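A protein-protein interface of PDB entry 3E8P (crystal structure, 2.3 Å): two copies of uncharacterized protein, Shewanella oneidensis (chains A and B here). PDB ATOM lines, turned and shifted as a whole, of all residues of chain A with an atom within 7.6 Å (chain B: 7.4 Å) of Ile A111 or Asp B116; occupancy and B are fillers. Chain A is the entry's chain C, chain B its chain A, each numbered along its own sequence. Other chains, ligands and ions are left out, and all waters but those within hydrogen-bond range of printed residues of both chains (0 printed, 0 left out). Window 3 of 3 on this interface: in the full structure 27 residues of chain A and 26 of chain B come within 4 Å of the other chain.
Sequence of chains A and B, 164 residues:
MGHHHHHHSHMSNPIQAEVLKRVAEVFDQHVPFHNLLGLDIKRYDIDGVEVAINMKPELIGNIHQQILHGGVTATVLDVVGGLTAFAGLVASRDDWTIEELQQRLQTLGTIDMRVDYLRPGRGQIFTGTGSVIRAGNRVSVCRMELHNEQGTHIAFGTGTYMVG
No position is printed for both chains.
N of Val B115 lies within hydrogen-bond range of O of Met A113, 2.8 Å away. NH2 of Arg B114 is in salt-bridge range of OD2 of Asp A112 (3.6 Å). N of Tyr B117 is in hydrogen-bond range of O of Ile A111 (2.9 Å).
The backbone NH (N) of Ile A111 lies within hydrogen-bond range of the backbone carbonyl oxygen (O) of Thr A160, 2.8 Å away. The guanidinium group (NH2) of Arg B114 is in salt-bridge range of the side-chain carboxylate (OD1) of Asp B116, 3.0 Å away. OD1 of Asp A78 lies within hydrogen-bond range of OG1 of Thr A110, at 2.7 Å. SD of Met A113 lies close to N of Asp A78 (3.7 Å). The backbone carbonyl oxygen of Thr B158 lies within hydrogen-bond range of the backbone NH of Arg B114 (3.0 Å). The backbone NH (N) of Asp B116 sits at hydrogen-bond distance from the backbone carbonyl oxygen (O) of Phe B156, 2.8 Å away.
Of the 13 printed residues of chain B, 4 touch a printed residue of chain A. Of the 14 printed residues of chain A, 4 touch a printed residue of chain B. Printed residues of chain A that touch a printed residue of chain B: Thr A110, Ile A111, Asp A112 and Met A113. Along chain A the printed residues that touch a printed residue of chain B span positions 110 to 113.
Asp B116 touches just these residues of chain A: Ile A111 and Asp A112. Printed residues of chain A within 4 Å of Arg B114: Asp A112 (3.6 Å) and Met A113 (3.1 Å). Printed residues of chain B within 4 Å of Met A113: Arg B114 (3.1 Å), Val B115 (2.8 Å) and Tyr B117 (3.97 Å). Ser A140 touches none of the printed residues of chain B. Thr A160 touches none of the printed residues of chain B. The nearest residue of chain B that does not touch Ile A111 is Val B115 (4.2 Å). The nearest residue of chain A that does not touch Asp B116 is Met A113 (5.2 Å). The nearest printed residue of chain B that does not touch Met A113 is Asp B116 (5.2 Å).
Among the printed residues, pairs that only touch across the chains: Thr A110 with Tyr B117, Ile A111 with Asp B116, Asp A112 with Val B115, Asp A112 with Asp B116, Met A113 with Arg B114 and Met A113 with Tyr B117.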
ATOM      1  N   ASP A  78      -6.299  10.434 -35.812  1.00  0.00           N
ATOM      2  CA  ASP A  78      -7.443  10.013 -35.006  1.00  0.00           C
ATOM      3  C   ASP A  78      -8.800  10.472 -35.579  1.00  0.00           C
ATOM      4  O   ASP A  78      -9.778   9.720 -35.570  1.00  0.00           O
ATOM      5  CB  ASP A  78      -7.270  10.537 -33.580  1.00  0.00           C
ATOM      6  CG  ASP A  78      -8.410  10.148 -32.671  1.00  0.00           C
ATOM      7  OD1 ASP A  78      -8.933   9.019 -32.807  1.00  0.00           O
ATOM      8  OD2 ASP A  78      -8.773  10.967 -31.802  1.00  0.00           O
ATOM      9  N   GLY A 109     -16.457   6.938 -30.896  1.00  0.00           N
ATOM     10  CA  GLY A 109     -15.337   7.324 -30.055  1.00  0.00           C
ATOM     11  C   GLY A 109     -14.161   6.392 -30.249  1.00  0.00           C
ATOM     12  O   GLY A 109     -14.326   5.254 -30.697  1.00  0.00           O
ATOM     13  N   THR A 110     -12.971   6.868 -29.902  1.00  0.00           N
ATOM     14  CA  THR A 110     -11.754   6.084 -30.046  1.00  0.00           C
ATOM     15  C   THR A 110     -11.498   5.260 -28.804  1.00  0.00           C
ATOM     16  O   THR A 110     -11.591   5.769 -27.690  1.00  0.00           O
ATOM     17  CB  THR A 110     -10.534   6.989 -30.249  1.00  0.00           C
ATOM     18  OG1 THR A 110     -10.835   7.962 -31.253  1.00  0.00           O
ATOM     19  CG2 THR A 110      -9.305   6.154 -30.685  1.00  0.00           C
ATOM     20  N   ILE A 111     -11.179   3.987 -28.993  1.00  0.00           N
ATOM     21  CA  ILE A 111     -10.883   3.115 -27.864  1.00  0.00           C
ATOM     22  C   ILE A 111      -9.364   3.133 -27.645  1.00  0.00           C
ATOM     23  O   ILE A 111      -8.886   3.413 -26.542  1.00  0.00           O
ATOM     24  CB  ILE A 111     -11.404   1.680 -28.127  1.00  0.00           C
ATOM     25  CG1 ILE A 111     -12.936   1.716 -28.226  1.00  0.00           C
ATOM     26  CG2 ILE A 111     -10.983   0.747 -27.003  1.00  0.00           C
ATOM     27  CD1 ILE A 111     -13.588   0.391 -28.586  1.00  0.00           C
ATOM     28  N   ASP A 112      -8.613   2.848 -28.705  1.00  0.00           N
ATOM     29  CA  ASP A 112      -7.158   2.884 -28.646  1.00  0.00           C
ATOM     30  C   ASP A 112      -6.634   3.293 -30.014  1.00  0.00           C
ATOM     31  O   ASP A 112      -7.325   3.154 -31.021  1.00  0.00           O
ATOM     32  CB  ASP A 112      -6.574   1.519 -28.237  1.00  0.00           C
ATOM     33  CG  ASP A 112      -6.718   0.456 -29.321  1.00  0.00           C
ATOM     34  OD1 ASP A 112      -6.083   0.591 -30.390  1.00  0.00           O
ATOM     35  OD2 ASP A 112      -7.468  -0.520 -29.096  1.00  0.00           O
ATOM     36  N   MET A 113      -5.415   3.811 -30.054  1.00  0.00           N
ATOM     37  CA  MET A 113      -4.830   4.214 -31.319  1.00  0.00           C
ATOM     38  C   MET A 113      -3.328   4.110 -31.260  1.00  0.00           C
ATOM     39  O   MET A 113      -2.722   4.392 -30.229  1.00  0.00           O
ATOM     40  CB  MET A 113      -5.207   5.661 -31.671  1.00  0.00           C
ATOM     41  CG  MET A 113      -4.429   6.189 -32.879  1.00  0.00           C
ATOM     42  SD  MET A 113      -4.832   8.019 -33.447  1.00  0.00           S
ATOM     43  CE  MET A 113      -4.243   8.939 -31.840  1.00  0.00           C
ATOM     44  N   ARG A 138     -20.431  -3.002 -33.647  1.00  0.00           N
ATOM     45  CA  ARG A 138     -20.083  -2.346 -32.387  1.00  0.00           C
ATOM     46  C   ARG A 138     -18.674  -1.745 -32.385  1.00  0.00           C
ATOM     47  O   ARG A 138     -18.461  -0.646 -31.875  1.00  0.00           O
ATOM     48  CB  ARG A 138     -20.206  -3.318 -31.210  1.00  0.00           C
ATOM     49  CG  ARG A 138     -21.627  -3.698 -30.852  1.00  0.00           C
ATOM     50  CD  ARG A 138     -21.748  -3.956 -29.356  1.00  0.00           C
ATOM     51  NE  ARG A 138     -23.098  -4.363 -28.978  1.00  0.00           N
ATOM     52  CZ  ARG A 138     -23.621  -5.550 -29.264  1.00  0.00           C
ATOM     53  NH1 ARG A 138     -22.905  -6.449 -29.929  1.00  0.00           N
ATOM     54  NH2 ARG A 138     -24.860  -5.840 -28.888  1.00  0.00           N
ATOM     55  N   VAL A 139     -17.714  -2.462 -32.960  1.00  0.00           N
ATOM     56  CA  VAL A 139     -16.341  -1.988 -33.005  1.00  0.00           C
ATOM     57  C   VAL A 139     -15.735  -2.131 -34.392  1.00  0.00           C
ATOM     58  O   VAL A 139     -15.961  -3.124 -35.072  1.00  0.00           O
ATOM     59  CB  VAL A 139     -15.452  -2.770 -32.009  1.00  0.00           C
ATOM     60  CG1 VAL A 139     -14.022  -2.244 -32.041  1.00  0.00           C
ATOM     61  CG2 VAL A 139     -16.013  -2.641 -30.619  1.00  0.00           C
ATOM     62  N   SER A 140     -14.973  -1.124 -34.809  1.00  0.00           N
ATOM     63  CA  SER A 140     -14.294  -1.146 -36.098  1.00  0.00           C
ATOM     64  C   SER A 140     -12.840  -0.757 -35.916  1.00  0.00           C
ATOM     65  O   SER A 140     -12.498   0.023 -35.021  1.00  0.00           O
ATOM     66  CB  SER A 140     -14.942  -0.178 -37.090  1.00  0.00           C
ATOM     67  OG  SER A 140     -16.198  -0.661 -37.528  1.00  0.00           O
ATOM     68  N   GLY A 159      -6.392   2.575 -35.666  1.00  0.00           N
ATOM     69  CA  GLY A 159      -7.281   2.898 -34.575  1.00  0.00           C
ATOM     70  C   GLY A 159      -8.451   1.948 -34.431  1.00  0.00           C
ATOM     71  O   GLY A 159      -8.969   1.430 -35.417  1.00  0.00           O
ATOM     72  N   THR A 160      -8.855   1.722 -33.187  1.00  0.00           N
ATOM     73  CA  THR A 160      -9.973   0.857 -32.856  1.00  0.00           C
ATOM     74  C   THR A 160     -11.048   1.815 -32.354  1.00  0.00           C
ATOM     75  O   THR A 160     -10.823   2.584 -31.420  1.00  0.00           O
ATOM     76  CB  THR A 160      -9.561  -0.144 -31.763  1.00  0.00           C
ATOM     77  OG1 THR A 160      -8.472  -0.946 -32.249  1.00  0.00           O
ATOM     78  CG2 THR A 160     -10.712  -1.034 -31.385  1.00  0.00           C
ATOM     79  N   TYR A 161     -12.213   1.773 -32.989  1.00  0.00           N
ATOM     80  CA  TYR A 161     -13.297   2.678 -32.650  1.00  0.00           C
ATOM     81  C   TYR A 161     -14.602   2.007 -32.266  1.00  0.00           C
ATOM     82  O   TYR A 161     -14.952   0.938 -32.777  1.00  0.00           O
ATOM     83  CB  TYR A 161     -13.575   3.597 -33.839  1.00  0.00           C
ATOM     84  CG  TYR A 161     -12.396   4.434 -34.250  1.00  0.00           C
ATOM     85  CD1 TYR A 161     -12.204   5.704 -33.716  1.00  0.00           C
ATOM     86  CD2 TYR A 161     -11.453   3.947 -35.149  1.00  0.00           C
ATOM     87  CE1 TYR A 161     -11.105   6.469 -34.061  1.00  0.00           C
ATOM     88  CE2 TYR A 161     -10.352   4.707 -35.503  1.00  0.00           C
ATOM     89  CZ  TYR A 161     -10.184   5.970 -34.952  1.00  0.00           C
ATOM     90  OH  TYR A 161      -9.093   6.737 -35.289  1.00  0.00           O
ATOM     91  N   MET A 162     -15.328   2.668 -31.373  1.00  0.00           N
ATOM     92  CA  MET A 162     -16.631   2.201 -30.931  1.00  0.00           C
ATOM     93  C   MET A 162     -17.627   2.852 -31.891  1.00  0.00           C
ATOM     94  O   MET A 162     -17.702   4.077 -31.963  1.00  0.00           O
ATOM     95  CB  MET A 162     -16.910   2.686 -29.510  1.00  0.00           C
ATOM     96  CG  MET A 162     -18.154   2.086 -28.899  1.00  0.00           C
ATOM     97  SD  MET A 162     -17.840   0.250 -28.445  1.00  0.00           S
ATOM     98  CE  MET A 162     -17.351   0.519 -26.582  1.00  0.00           C
ATOM     99  N   VAL A 163     -18.373   2.040 -32.634  1.00  0.00           N
ATOM    100  CA  VAL A 163     -19.349   2.559 -33.592  1.00  0.00           C
ATOM    101  C   VAL A 163     -20.768   2.189 -33.179  1.00  0.00           C
ATOM    102  O   VAL A 163     -21.719   2.329 -33.954  1.00  0.00           O
ATOM    103  CB  VAL A 163     -19.079   2.012 -35.017  1.00  0.00           C
ATOM    104  CG1 VAL A 163     -17.776   2.578 -35.550  1.00  0.00           C
ATOM    105  CG2 VAL A 163     -19.017   0.493 -34.990  1.00  0.00           C
ATOM    106  N   THR B  73      -5.236  15.002 -25.589  1.00  0.00           N
ATOM    107  CA  THR B  73      -4.801  13.933 -24.698  1.00  0.00           C
ATOM    108  C   THR B  73      -3.568  13.241 -25.293  1.00  0.00           C
ATOM    109  O   THR B  73      -2.590  12.997 -24.590  1.00  0.00           O
ATOM    110  CB  THR B  73      -5.931  12.918 -24.489  1.00  0.00           C
ATOM    111  OG1 THR B  73      -7.031  13.566 -23.837  1.00  0.00           O
ATOM    112  CG2 THR B  73      -5.459  11.767 -23.643  1.00  0.00           C
ATOM    113  N   LEU B  77       0.300  13.152 -23.678  1.00  0.00           N
ATOM    114  CA  LEU B  77       0.928  11.870 -23.393  1.00  0.00           C
ATOM    115  C   LEU B  77       2.253  11.702 -24.132  1.00  0.00           C
ATOM    116  O   LEU B  77       3.205  11.154 -23.573  1.00  0.00           O
ATOM    117  CB  LEU B  77      -0.022  10.722 -23.748  1.00  0.00           C
ATOM    118  CG  LEU B  77      -1.262  10.578 -22.859  1.00  0.00           C
ATOM    119  CD1 LEU B  77      -2.253   9.611 -23.497  1.00  0.00           C
ATOM    120  CD2 LEU B  77      -0.850  10.084 -21.495  1.00  0.00           C
ATOM    121  N   ARG B 114       1.064   4.375 -28.492  1.00  0.00           N
ATOM    122  CA  ARG B 114      -0.262   3.805 -28.370  1.00  0.00           C
ATOM    123  C   ARG B 114      -0.972   4.538 -27.248  1.00  0.00           C
ATOM    124  O   ARG B 114      -0.442   4.679 -26.150  1.00  0.00           O
ATOM    125  CB  ARG B 114      -0.211   2.317 -28.017  1.00  0.00           C
ATOM    126  CG  ARG B 114      -1.586   1.759 -27.644  1.00  0.00           C
ATOM    127  CD  ARG B 114      -1.503   0.350 -27.067  1.00  0.00           C
ATOM    128  NE  ARG B 114      -2.817  -0.160 -26.681  1.00  0.00           N
ATOM    129  CZ  ARG B 114      -3.574  -0.970 -27.423  1.00  0.00           C
ATOM    130  NH1 ARG B 114      -3.161  -1.388 -28.617  1.00  0.00           N
ATOM    131  NH2 ARG B 114      -4.758  -1.369 -26.965  1.00  0.00           N
ATOM    132  N   VAL B 115      -2.174   5.013 -27.529  1.00  0.00           N
ATOM    133  CA  VAL B 115      -2.951   5.694 -26.522  1.00  0.00           C
ATOM    134  C   VAL B 115      -4.205   4.881 -26.254  1.00  0.00           C
ATOM    135  O   VAL B 115      -4.892   4.450 -27.188  1.00  0.00           O
ATOM    136  CB  VAL B 115      -3.374   7.092 -26.994  1.00  0.00           C
ATOM    137  CG1 VAL B 115      -4.248   7.748 -25.942  1.00  0.00           C
ATOM    138  CG2 VAL B 115      -2.147   7.937 -27.276  1.00  0.00           C
ATOM    139  N   ASP B 116      -4.496   4.657 -24.984  1.00  0.00           N
ATOM    140  CA  ASP B 116      -5.698   3.929 -24.594  1.00  0.00           C
ATOM    141  C   ASP B 116      -6.622   4.945 -23.909  1.00  0.00           C
ATOM    142  O   ASP B 116      -6.286   5.484 -22.850  1.00  0.00           O
ATOM    143  CB  ASP B 116      -5.337   2.778 -23.639  1.00  0.00           C
ATOM    144  CG  ASP B 116      -4.693   1.588 -24.367  1.00  0.00           C
ATOM    145  OD1 ASP B 116      -5.390   0.886 -25.136  1.00  0.00           O
ATOM    146  OD2 ASP B 116      -3.486   1.355 -24.170  1.00  0.00           O
ATOM    147  N   TYR B 117      -7.757   5.226 -24.546  1.00  0.00           N
ATOM    148  CA  TYR B 117      -8.751   6.166 -24.028  1.00  0.00           C
ATOM    149  C   TYR B 117      -9.665   5.419 -23.072  1.00  0.00           C
ATOM    150  O   TYR B 117     -10.506   4.629 -23.479  1.00  0.00           O
ATOM    151  CB  TYR B 117      -9.556   6.774 -25.186  1.00  0.00           C
ATOM    152  CG  TYR B 117      -8.702   7.613 -26.124  1.00  0.00           C
ATOM    153  CD1 TYR B 117      -8.086   7.053 -27.242  1.00  0.00           C
ATOM    154  CD2 TYR B 117      -8.463   8.956 -25.857  1.00  0.00           C
ATOM    155  CE1 TYR B 117      -7.253   7.822 -28.066  1.00  0.00           C
ATOM    156  CE2 TYR B 117      -7.638   9.720 -26.664  1.00  0.00           C
ATOM    157  CZ  TYR B 117      -7.036   9.155 -27.763  1.00  0.00           C
ATOM    158  OH  TYR B 117      -6.203   9.929 -28.536  1.00  0.00           O
ATOM    159  N   LEU B 118      -9.495   5.682 -21.787  1.00  0.00           N
ATOM    160  CA  LEU B 118     -10.256   4.989 -20.751  1.00  0.00           C
ATOM    161  C   LEU B 118     -11.676   5.497 -20.531  1.00  0.00           C
ATOM    162  O   LEU B 118     -12.600   4.701 -20.381  1.00  0.00           O
ATOM    163  CB  LEU B 118      -9.472   5.050 -19.430  1.00  0.00           C
ATOM    164  CG  LEU B 118      -7.993   4.675 -19.579  1.00  0.00           C
ATOM    165  CD1 LEU B 118      -7.235   5.002 -18.312  1.00  0.00           C
ATOM    166  CD2 LEU B 118      -7.885   3.191 -19.922  1.00  0.00           C
ATOM    167  N   ARG B 119     -11.844   6.815 -20.497  1.00  0.00           N
ATOM    168  CA  ARG B 119     -13.154   7.429 -20.274  1.00  0.00           C
ATOM    169  C   ARG B 119     -13.111   8.901 -20.682  1.00  0.00           C
ATOM    170  O   ARG B 119     -12.037   9.481 -20.785  1.00  0.00           O
ATOM    171  CB  ARG B 119     -13.553   7.286 -18.800  1.00  0.00           C
ATOM    172  CG  ARG B 119     -12.507   7.804 -17.812  1.00  0.00           C
ATOM    173  CD  ARG B 119     -12.925   7.497 -16.388  1.00  0.00           C
ATOM    174  NE  ARG B 119     -12.966   6.059 -16.153  1.00  0.00           N
ATOM    175  CZ  ARG B 119     -11.918   5.326 -15.794  1.00  0.00           C
ATOM    176  NH1 ARG B 119     -10.735   5.894 -15.613  1.00  0.00           N
ATOM    177  NH2 ARG B 119     -12.046   4.015 -15.638  1.00  0.00           N
ATOM    178  N   ILE B 154      -7.811   9.574 -17.221  1.00  0.00           N
ATOM    179  CA  ILE B 154      -8.466   9.866 -18.483  1.00  0.00           C
ATOM    180  C   ILE B 154      -7.979   8.932 -19.572  1.00  0.00           C
ATOM    181  O   ILE B 154      -8.776   8.339 -20.304  1.00  0.00           O
ATOM    182  CB  ILE B 154      -8.189  11.327 -18.907  1.00  0.00           C
ATOM    183  CG1 ILE B 154      -8.673  12.273 -17.813  1.00  0.00           C
ATOM    184  CG2 ILE B 154      -8.906  11.648 -20.191  1.00  0.00           C
ATOM    185  CD1 ILE B 154     -10.155  12.124 -17.479  1.00  0.00           C
ATOM    186  N   ALA B 155      -6.664   8.794 -19.668  1.00  0.00           N
ATOM    187  CA  ALA B 155      -6.066   7.936 -20.677  1.00  0.00           C
ATOM    188  C   ALA B 155      -4.680   7.480 -20.251  1.00  0.00           C
ATOM    189  O   ALA B 155      -4.043   8.121 -19.417  1.00  0.00           O
ATOM    190  CB  ALA B 155      -5.973   8.681 -22.000  1.00  0.00           C
ATOM    191  N   PHE B 156      -4.238   6.358 -20.821  1.00  0.00           N
ATOM    192  CA  PHE B 156      -2.912   5.823 -20.563  1.00  0.00           C
ATOM    193  C   PHE B 156      -2.207   5.798 -21.903  1.00  0.00           C
ATOM    194  O   PHE B 156      -2.844   5.713 -22.950  1.00  0.00           O
ATOM    195  CB  PHE B 156      -2.947   4.379 -20.046  1.00  0.00           C
ATOM    196  CG  PHE B 156      -3.495   4.224 -18.659  1.00  0.00           C
ATOM    197  CD1 PHE B 156      -3.455   5.270 -17.744  1.00  0.00           C
ATOM    198  CD2 PHE B 156      -3.987   2.992 -18.246  1.00  0.00           C
ATOM    199  CE1 PHE B 156      -3.894   5.088 -16.428  1.00  0.00           C
ATOM    200  CE2 PHE B 156      -4.424   2.793 -16.947  1.00  0.00           C
ATOM    201  CZ  PHE B 156      -4.378   3.854 -16.026  1.00  0.00           C
ATOM    202  N   GLY B 157      -0.884   5.853 -21.867  1.00  0.00           N
ATOM    203  CA  GLY B 157      -0.119   5.799 -23.094  1.00  0.00           C
ATOM    204  C   GLY B 157       1.125   4.938 -22.933  1.00  0.00           C
ATOM    205  O   GLY B 157       1.513   4.575 -21.822  1.00  0.00           O
ATOM    206  N   THR B 158       1.728   4.579 -24.057  1.00  0.00           N
ATOM    207  CA  THR B 158       2.973   3.821 -24.070  1.00  0.00           C
ATOM    208  C   THR B 158       3.707   4.352 -25.296  1.00  0.00           C
ATOM    209  O   THR B 158       3.162   4.339 -26.403  1.00  0.00           O
ATOM    210  CB  THR B 158       2.738   2.297 -24.222  1.00  0.00           C
ATOM    211  OG1 THR B 158       1.926   1.831 -23.143  1.00  0.00           O
ATOM    212  CG2 THR B 158       4.060   1.529 -24.200  1.00  0.00           C
